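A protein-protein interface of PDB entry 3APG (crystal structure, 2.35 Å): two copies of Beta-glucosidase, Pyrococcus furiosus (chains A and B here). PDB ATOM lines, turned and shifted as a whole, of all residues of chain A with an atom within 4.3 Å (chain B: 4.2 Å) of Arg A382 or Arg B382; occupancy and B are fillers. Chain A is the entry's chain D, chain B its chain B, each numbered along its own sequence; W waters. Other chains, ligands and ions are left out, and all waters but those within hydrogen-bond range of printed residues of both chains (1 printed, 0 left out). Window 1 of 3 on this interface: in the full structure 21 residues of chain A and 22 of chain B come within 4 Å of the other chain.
Gly A333 touches Arg B472, and with the chains exchanged Arg A472 touches Gly B333.
Arg B382 touches its own counterpart, Arg A382.
Arg A382 touches Tyr B383, and with the chains exchanged Tyr A383 touches Arg B382.
Arg A382 touches Arg B472, and with the chains exchanged Arg A472 touches Arg B382.
Positions printed for both chains: 333, 378, 380, 381, 382, 383, 384 and 472.
The backbone carbonyl oxygen (O) of Gly B333 is in hydrogen-bond range of the guanidinium group (NH2) of Arg A472, 2.8 Å away.
The guanidinium group (NH1) of Arg B382 is in hydrogen-bond range of the side-chain hydroxyl (OH) of Tyr A383.
The side-chain hydroxyl (OH) of Tyr B383 is in hydrogen-bond range of the guanidinium group (NH1) of Arg A382.
The guanidinium group of Arg B472 is in hydrogen-bond range of the backbone carbonyl oxygen of Gly A333.
NH2 of Arg A472 sits close to NH2 of Arg B382 (3.4 Å).
Asp A378 touches none of the printed residues of chain B.
Arg A382 touches just these residues of chain B: Arg B382, Tyr B383 and Arg B472.
Of the printed residues of chain B, Tyr A383 touches Arg B382 (2.8 Å).
Printed residues of chain B within 4 Å of Arg A472: Gly B333 (2.8 Å) and Arg B382 (3.4 Å).
Asp B381 touches none of the printed residues of chain A.
Arg B382 touches three residues of chain A.
Printed residues of chain A within 4 Å of Arg B472: Gly A333 (2.7 Å) and Arg A382 (3.96 Å).
The nearest printed residue of chain B that does not touch Arg A382 is Asp B381 (4.4 Å).
NH2 of Arg B382 sits at hydrogen-bond distance from O of Gly B333, at 3.1 Å.
N of Arg B382 is in hydrogen-bond range of OD2 of Asp B378.
The side-chain carboxylate (OD2) of Asp B378 is in hydrogen-bond range of the backbone NH (N) of Tyr B383, at 2.7 Å.
O of Gly A333 is in hydrogen-bond range of NH2 of Arg A382 (3.0 Å).
The backbone NH of Arg A382 sits at hydrogen-bond distance from the side-chain carboxylate of Asp A378 (3.1 Å).
The backbone NH (N) of Tyr A383 lies within hydrogen-bond range of the side-chain carboxylate (OD2) of Asp A378, at 2.7 Å.
Water W1 bridges the side-chain hydroxyl (OH) of Tyr A383 (2.7 Å) and the guanidinium group (NH1) of Arg B382 (3.5 Å).
Among the printed residues, pairs that only touch across the chains: Arg A382 with Arg B382 (3.4 Å) and Arg A382 with Arg B472 (3.96 Å).
Along chain B the printed residues that touch a printed residue of chain A span positions 333 to 472.
Of the 8 printed residues of chain A, 4 touch a printed residue of chain B.
Printed residues of chain A that touch a printed residue of chain B: Gly A333, Arg A382, Tyr A383 and Arg A472.
Hydrophobic or aromatic side chains of chain A within 4 Å of the printed part of chain B: Tyr A383.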
ATOM      1  N   GLY A 333     -33.318 -23.237 -19.514  1.00  0.00           N
ATOM      2  CA  GLY A 333     -32.327 -22.986 -18.495  1.00  0.00           C
ATOM      3  C   GLY A 333     -32.798 -21.892 -17.584  1.00  0.00           C
ATOM      4  O   GLY A 333     -32.015 -21.450 -16.757  1.00  0.00           O
ATOM      5  N   ASP A 378     -30.076 -31.307 -17.699  1.00  0.00           N
ATOM      6  CA  ASP A 378     -29.528 -30.443 -16.697  1.00  0.00           C
ATOM      7  C   ASP A 378     -28.082 -30.783 -16.574  1.00  0.00           C
ATOM      8  O   ASP A 378     -27.728 -31.641 -15.778  1.00  0.00           O
ATOM      9  CB  ASP A 378     -30.274 -30.686 -15.363  1.00  0.00           C
ATOM     10  CG  ASP A 378     -29.683 -29.945 -14.194  1.00  0.00           C
ATOM     11  OD1 ASP A 378     -28.771 -29.130 -14.402  1.00  0.00           O
ATOM     12  OD2 ASP A 378     -30.164 -30.161 -13.062  1.00  0.00           O
ATOM     13  N   ALA A 380     -25.537 -29.202 -15.223  1.00  0.00           N
ATOM     14  CA  ALA A 380     -24.727 -28.835 -14.049  1.00  0.00           C
ATOM     15  C   ALA A 380     -25.305 -29.524 -12.811  1.00  0.00           C
ATOM     16  O   ALA A 380     -24.847 -29.335 -11.667  1.00  0.00           O
ATOM     17  CB  ALA A 380     -24.762 -27.360 -13.856  1.00  0.00           C
ATOM     18  N   ASP A 381     -26.344 -30.305 -13.053  1.00  0.00           N
ATOM     19  CA  ASP A 381     -27.030 -30.983 -11.972  1.00  0.00           C
ATOM     20  C   ASP A 381     -27.578 -29.965 -10.956  1.00  0.00           C
ATOM     21  O   ASP A 381     -27.737 -30.315  -9.835  1.00  0.00           O
ATOM     22  CB  ASP A 381     -26.123 -32.049 -11.277  1.00  0.00           C
ATOM     23  CG  ASP A 381     -26.931 -33.232 -10.596  1.00  0.00           C
ATOM     24  OD1 ASP A 381     -27.744 -33.897 -11.272  1.00  0.00           O
ATOM     25  OD2 ASP A 381     -26.705 -33.522  -9.392  1.00  0.00           O
ATOM     26  N   ARG A 382     -27.936 -28.755 -11.378  1.00  0.00           N
ATOM     27  CA  ARG A 382     -28.610 -27.753 -10.540  1.00  0.00           C
ATOM     28  C   ARG A 382     -29.996 -28.215  -9.953  1.00  0.00           C
ATOM     29  O   ARG A 382     -30.378 -27.821  -8.855  1.00  0.00           O
ATOM     30  CB  ARG A 382     -28.933 -26.578 -11.429  1.00  0.00           C
ATOM     31  CG  ARG A 382     -27.765 -25.944 -12.059  1.00  0.00           C
ATOM     32  CD  ARG A 382     -28.089 -24.491 -12.535  1.00  0.00           C
ATOM     33  NE  ARG A 382     -29.035 -24.465 -13.669  1.00  0.00           N
ATOM     34  CZ  ARG A 382     -29.697 -23.387 -14.069  1.00  0.00           C
ATOM     35  NH1 ARG A 382     -29.476 -22.220 -13.445  1.00  0.00           N
ATOM     36  NH2 ARG A 382     -30.571 -23.480 -15.067  1.00  0.00           N
ATOM     37  N   TYR A 383     -30.782 -28.967 -10.716  1.00  0.00           N
ATOM     38  CA  TYR A 383     -32.173 -29.118 -10.331  1.00  0.00           C
ATOM     39  C   TYR A 383     -32.576 -30.590 -10.229  1.00  0.00           C
ATOM     40  O   TYR A 383     -33.564 -30.965  -9.573  1.00  0.00           O
ATOM     41  CB  TYR A 383     -33.090 -28.343 -11.300  1.00  0.00           C
ATOM     42  CG  TYR A 383     -32.968 -26.810 -11.230  1.00  0.00           C
ATOM     43  CD1 TYR A 383     -33.252 -26.117 -10.040  1.00  0.00           C
ATOM     44  CD2 TYR A 383     -32.658 -26.047 -12.371  1.00  0.00           C
ATOM     45  CE1 TYR A 383     -33.233 -24.693  -9.994  1.00  0.00           C
ATOM     46  CE2 TYR A 383     -32.585 -24.628 -12.316  1.00  0.00           C
ATOM     47  CZ  TYR A 383     -32.874 -23.959 -11.117  1.00  0.00           C
ATOM     48  OH  TYR A 383     -32.807 -22.569 -11.051  1.00  0.00           O
ATOM     49  N   ARG A 384     -31.753 -31.438 -10.815  1.00  0.00           N
ATOM     50  CA  ARG A 384     -32.056 -32.882 -10.905  1.00  0.00           C
ATOM     51  C   ARG A 384     -32.240 -33.553  -9.544  1.00  0.00           C
ATOM     52  O   ARG A 384     -33.167 -34.323  -9.404  1.00  0.00           O
ATOM     53  CB  ARG A 384     -31.075 -33.610 -11.815  1.00  0.00           C
ATOM     54  CG  ARG A 384     -31.235 -35.055 -11.763  1.00  0.00           C
ATOM     55  CD  ARG A 384     -30.268 -35.733 -12.691  1.00  0.00           C
ATOM     56  NE  ARG A 384     -30.350 -35.319 -14.073  1.00  0.00           N
ATOM     57  CZ  ARG A 384     -29.458 -34.521 -14.691  1.00  0.00           C
ATOM     58  NH1 ARG A 384     -28.435 -33.983 -14.013  1.00  0.00           N
ATOM     59  NH2 ARG A 384     -29.590 -34.251 -16.009  1.00  0.00           N
ATOM     60  N   ARG A 472     -39.439 -19.375  -7.869  1.00  0.00           N
ATOM     61  CA  ARG A 472     -39.522 -17.916  -7.624  1.00  0.00           C
ATOM     62  C   ARG A 472     -40.948 -17.312  -7.830  1.00  0.00           C
ATOM     63  O   ARG A 472     -41.623 -17.588  -8.837  1.00  0.00           O
ATOM     64  CB  ARG A 472     -38.484 -17.248  -8.536  1.00  0.00           C
ATOM     65  CG  ARG A 472     -37.060 -17.773  -8.284  1.00  0.00           C
ATOM     66  CD  ARG A 472     -36.013 -16.885  -8.980  1.00  0.00           C
ATOM     67  NE  ARG A 472     -34.610 -17.290  -8.726  1.00  0.00           N
ATOM     68  CZ  ARG A 472     -33.548 -16.828  -9.413  1.00  0.00           C
ATOM     69  NH1 ARG A 472     -33.716 -15.946 -10.394  1.00  0.00           N
ATOM     70  NH2 ARG A 472     -32.311 -17.243  -9.124  1.00  0.00           N
ATOM     71  N   GLY B 333     -28.889 -14.561  -7.050  1.00  0.00           N
ATOM     72  CA  GLY B 333     -29.528 -15.642  -7.681  1.00  0.00           C
ATOM     73  C   GLY B 333     -29.210 -15.745  -9.143  1.00  0.00           C
ATOM     74  O   GLY B 333     -29.677 -16.655  -9.774  1.00  0.00           O
ATOM     75  N   ASP B 378     -27.244 -20.651  -0.729  1.00  0.00           N
ATOM     76  CA  ASP B 378     -27.824 -21.444  -1.820  1.00  0.00           C
ATOM     77  C   ASP B 378     -28.982 -22.318  -1.319  1.00  0.00           C
ATOM     78  O   ASP B 378     -28.787 -23.467  -0.940  1.00  0.00           O
ATOM     79  CB  ASP B 378     -26.716 -22.264  -2.467  1.00  0.00           C
ATOM     80  CG  ASP B 378     -27.217 -23.143  -3.613  1.00  0.00           C
ATOM     81  OD1 ASP B 378     -28.419 -23.017  -3.956  1.00  0.00           O
ATOM     82  OD2 ASP B 378     -26.395 -23.953  -4.187  1.00  0.00           O
ATOM     83  N   ALA B 380     -31.278 -23.959  -2.392  1.00  0.00           N
ATOM     84  CA  ALA B 380     -31.772 -25.156  -3.042  1.00  0.00           C
ATOM     85  C   ALA B 380     -30.617 -26.084  -3.447  1.00  0.00           C
ATOM     86  O   ALA B 380     -30.831 -27.086  -4.143  1.00  0.00           O
ATOM     87  CB  ALA B 380     -32.569 -24.767  -4.242  1.00  0.00           C
ATOM     88  N   ASP B 381     -29.394 -25.750  -3.043  1.00  0.00           N
ATOM     89  CA  ASP B 381     -28.226 -26.582  -3.424  1.00  0.00           C
ATOM     90  C   ASP B 381     -28.040 -26.655  -4.950  1.00  0.00           C
ATOM     91  O   ASP B 381     -27.582 -27.684  -5.493  1.00  0.00           O
ATOM     92  CB  ASP B 381     -28.358 -27.993  -2.812  1.00  0.00           C
ATOM     93  CG  ASP B 381     -27.062 -28.524  -2.215  1.00  0.00           C
ATOM     94  OD1 ASP B 381     -26.293 -27.754  -1.531  1.00  0.00           O
ATOM     95  OD2 ASP B 381     -26.847 -29.751  -2.387  1.00  0.00           O
ATOM     96  N   ARG B 382     -28.403 -25.569  -5.652  1.00  0.00           N
ATOM     97  CA  ARG B 382     -28.226 -25.543  -7.119  1.00  0.00           C
ATOM     98  C   ARG B 382     -26.753 -25.635  -7.439  1.00  0.00           C
ATOM     99  O   ARG B 382     -26.394 -26.277  -8.372  1.00  0.00           O
ATOM    100  CB  ARG B 382     -28.736 -24.247  -7.703  1.00  0.00           C
ATOM    101  CG  ARG B 382     -30.136 -24.022  -7.407  1.00  0.00           C
ATOM    102  CD  ARG B 382     -30.701 -22.971  -8.280  1.00  0.00           C
ATOM    103  NE  ARG B 382     -30.193 -21.641  -7.982  1.00  0.00           N
ATOM    104  CZ  ARG B 382     -30.326 -20.641  -8.844  1.00  0.00           C
ATOM    105  NH1 ARG B 382     -30.913 -20.856 -10.025  1.00  0.00           N
ATOM    106  NH2 ARG B 382     -29.824 -19.451  -8.553  1.00  0.00           N
ATOM    107  N   TYR B 383     -25.914 -25.027  -6.616  1.00  0.00           N
ATOM    108  CA  TYR B 383     -24.517 -24.747  -6.986  1.00  0.00           C
ATOM    109  C   TYR B 383     -23.503 -25.161  -5.926  1.00  0.00           C
ATOM    110  O   TYR B 383     -22.304 -25.182  -6.193  1.00  0.00           O
ATOM    111  CB  TYR B 383     -24.328 -23.240  -7.232  1.00  0.00           C
ATOM    112  CG  TYR B 383     -25.029 -22.731  -8.460  1.00  0.00           C
ATOM    113  CD1 TYR B 383     -24.719 -23.245  -9.733  1.00  0.00           C
ATOM    114  CD2 TYR B 383     -26.027 -21.730  -8.370  1.00  0.00           C
ATOM    115  CE1 TYR B 383     -25.376 -22.780 -10.856  1.00  0.00           C
ATOM    116  CE2 TYR B 383     -26.683 -21.270  -9.516  1.00  0.00           C
ATOM    117  CZ  TYR B 383     -26.363 -21.766 -10.749  1.00  0.00           C
ATOM    118  OH  TYR B 383     -26.998 -21.273 -11.911  1.00  0.00           O
ATOM    119  N   ARG B 384     -23.967 -25.476  -4.723  1.00  0.00           N
ATOM    120  CA  ARG B 384     -23.044 -25.812  -3.665  1.00  0.00           C
ATOM    121  C   ARG B 384     -22.152 -27.037  -3.960  1.00  0.00           C
ATOM    122  O   ARG B 384     -20.976 -27.022  -3.606  1.00  0.00           O
ATOM    123  CB  ARG B 384     -23.758 -25.945  -2.328  1.00  0.00           C
ATOM    124  CG  ARG B 384     -22.845 -25.804  -1.123  1.00  0.00           C
ATOM    125  CD  ARG B 384     -23.654 -25.976   0.166  1.00  0.00           C
ATOM    126  NE  ARG B 384     -24.344 -24.729   0.597  1.00  0.00           N
ATOM    127  CZ  ARG B 384     -25.661 -24.483   0.462  1.00  0.00           C
ATOM    128  NH1 ARG B 384     -26.509 -25.350  -0.114  1.00  0.00           N
ATOM    129  NH2 ARG B 384     -26.153 -23.371   0.934  1.00  0.00           N
ATOM    130  N   ARG B 472     -22.303 -19.398 -17.881  1.00  0.00           N
ATOM    131  CA  ARG B 472     -22.830 -18.878 -19.151  1.00  0.00           C
ATOM    132  C   ARG B 472     -21.858 -17.818 -19.832  1.00  0.00           C
ATOM    133  O   ARG B 472     -21.952 -16.584 -19.675  1.00  0.00           O
ATOM    134  CB  ARG B 472     -24.243 -18.294 -18.885  1.00  0.00           C
ATOM    135  CG  ARG B 472     -25.430 -19.311 -18.663  1.00  0.00           C
ATOM    136  CD  ARG B 472     -26.806 -18.550 -18.997  1.00  0.00           C
ATOM    137  NE  ARG B 472     -28.117 -18.980 -18.407  1.00  0.00           N
ATOM    138  CZ  ARG B 472     -28.363 -20.120 -17.764  1.00  0.00           C
ATOM    139  NH1 ARG B 472     -27.399 -21.024 -17.581  1.00  0.00           N
ATOM    140  NH2 ARG B 472     -29.573 -20.356 -17.291  1.00  0.00           N
HETATM  141  O   HOH W   1     -33.847 -22.065  -8.625  1.00  0.00           O
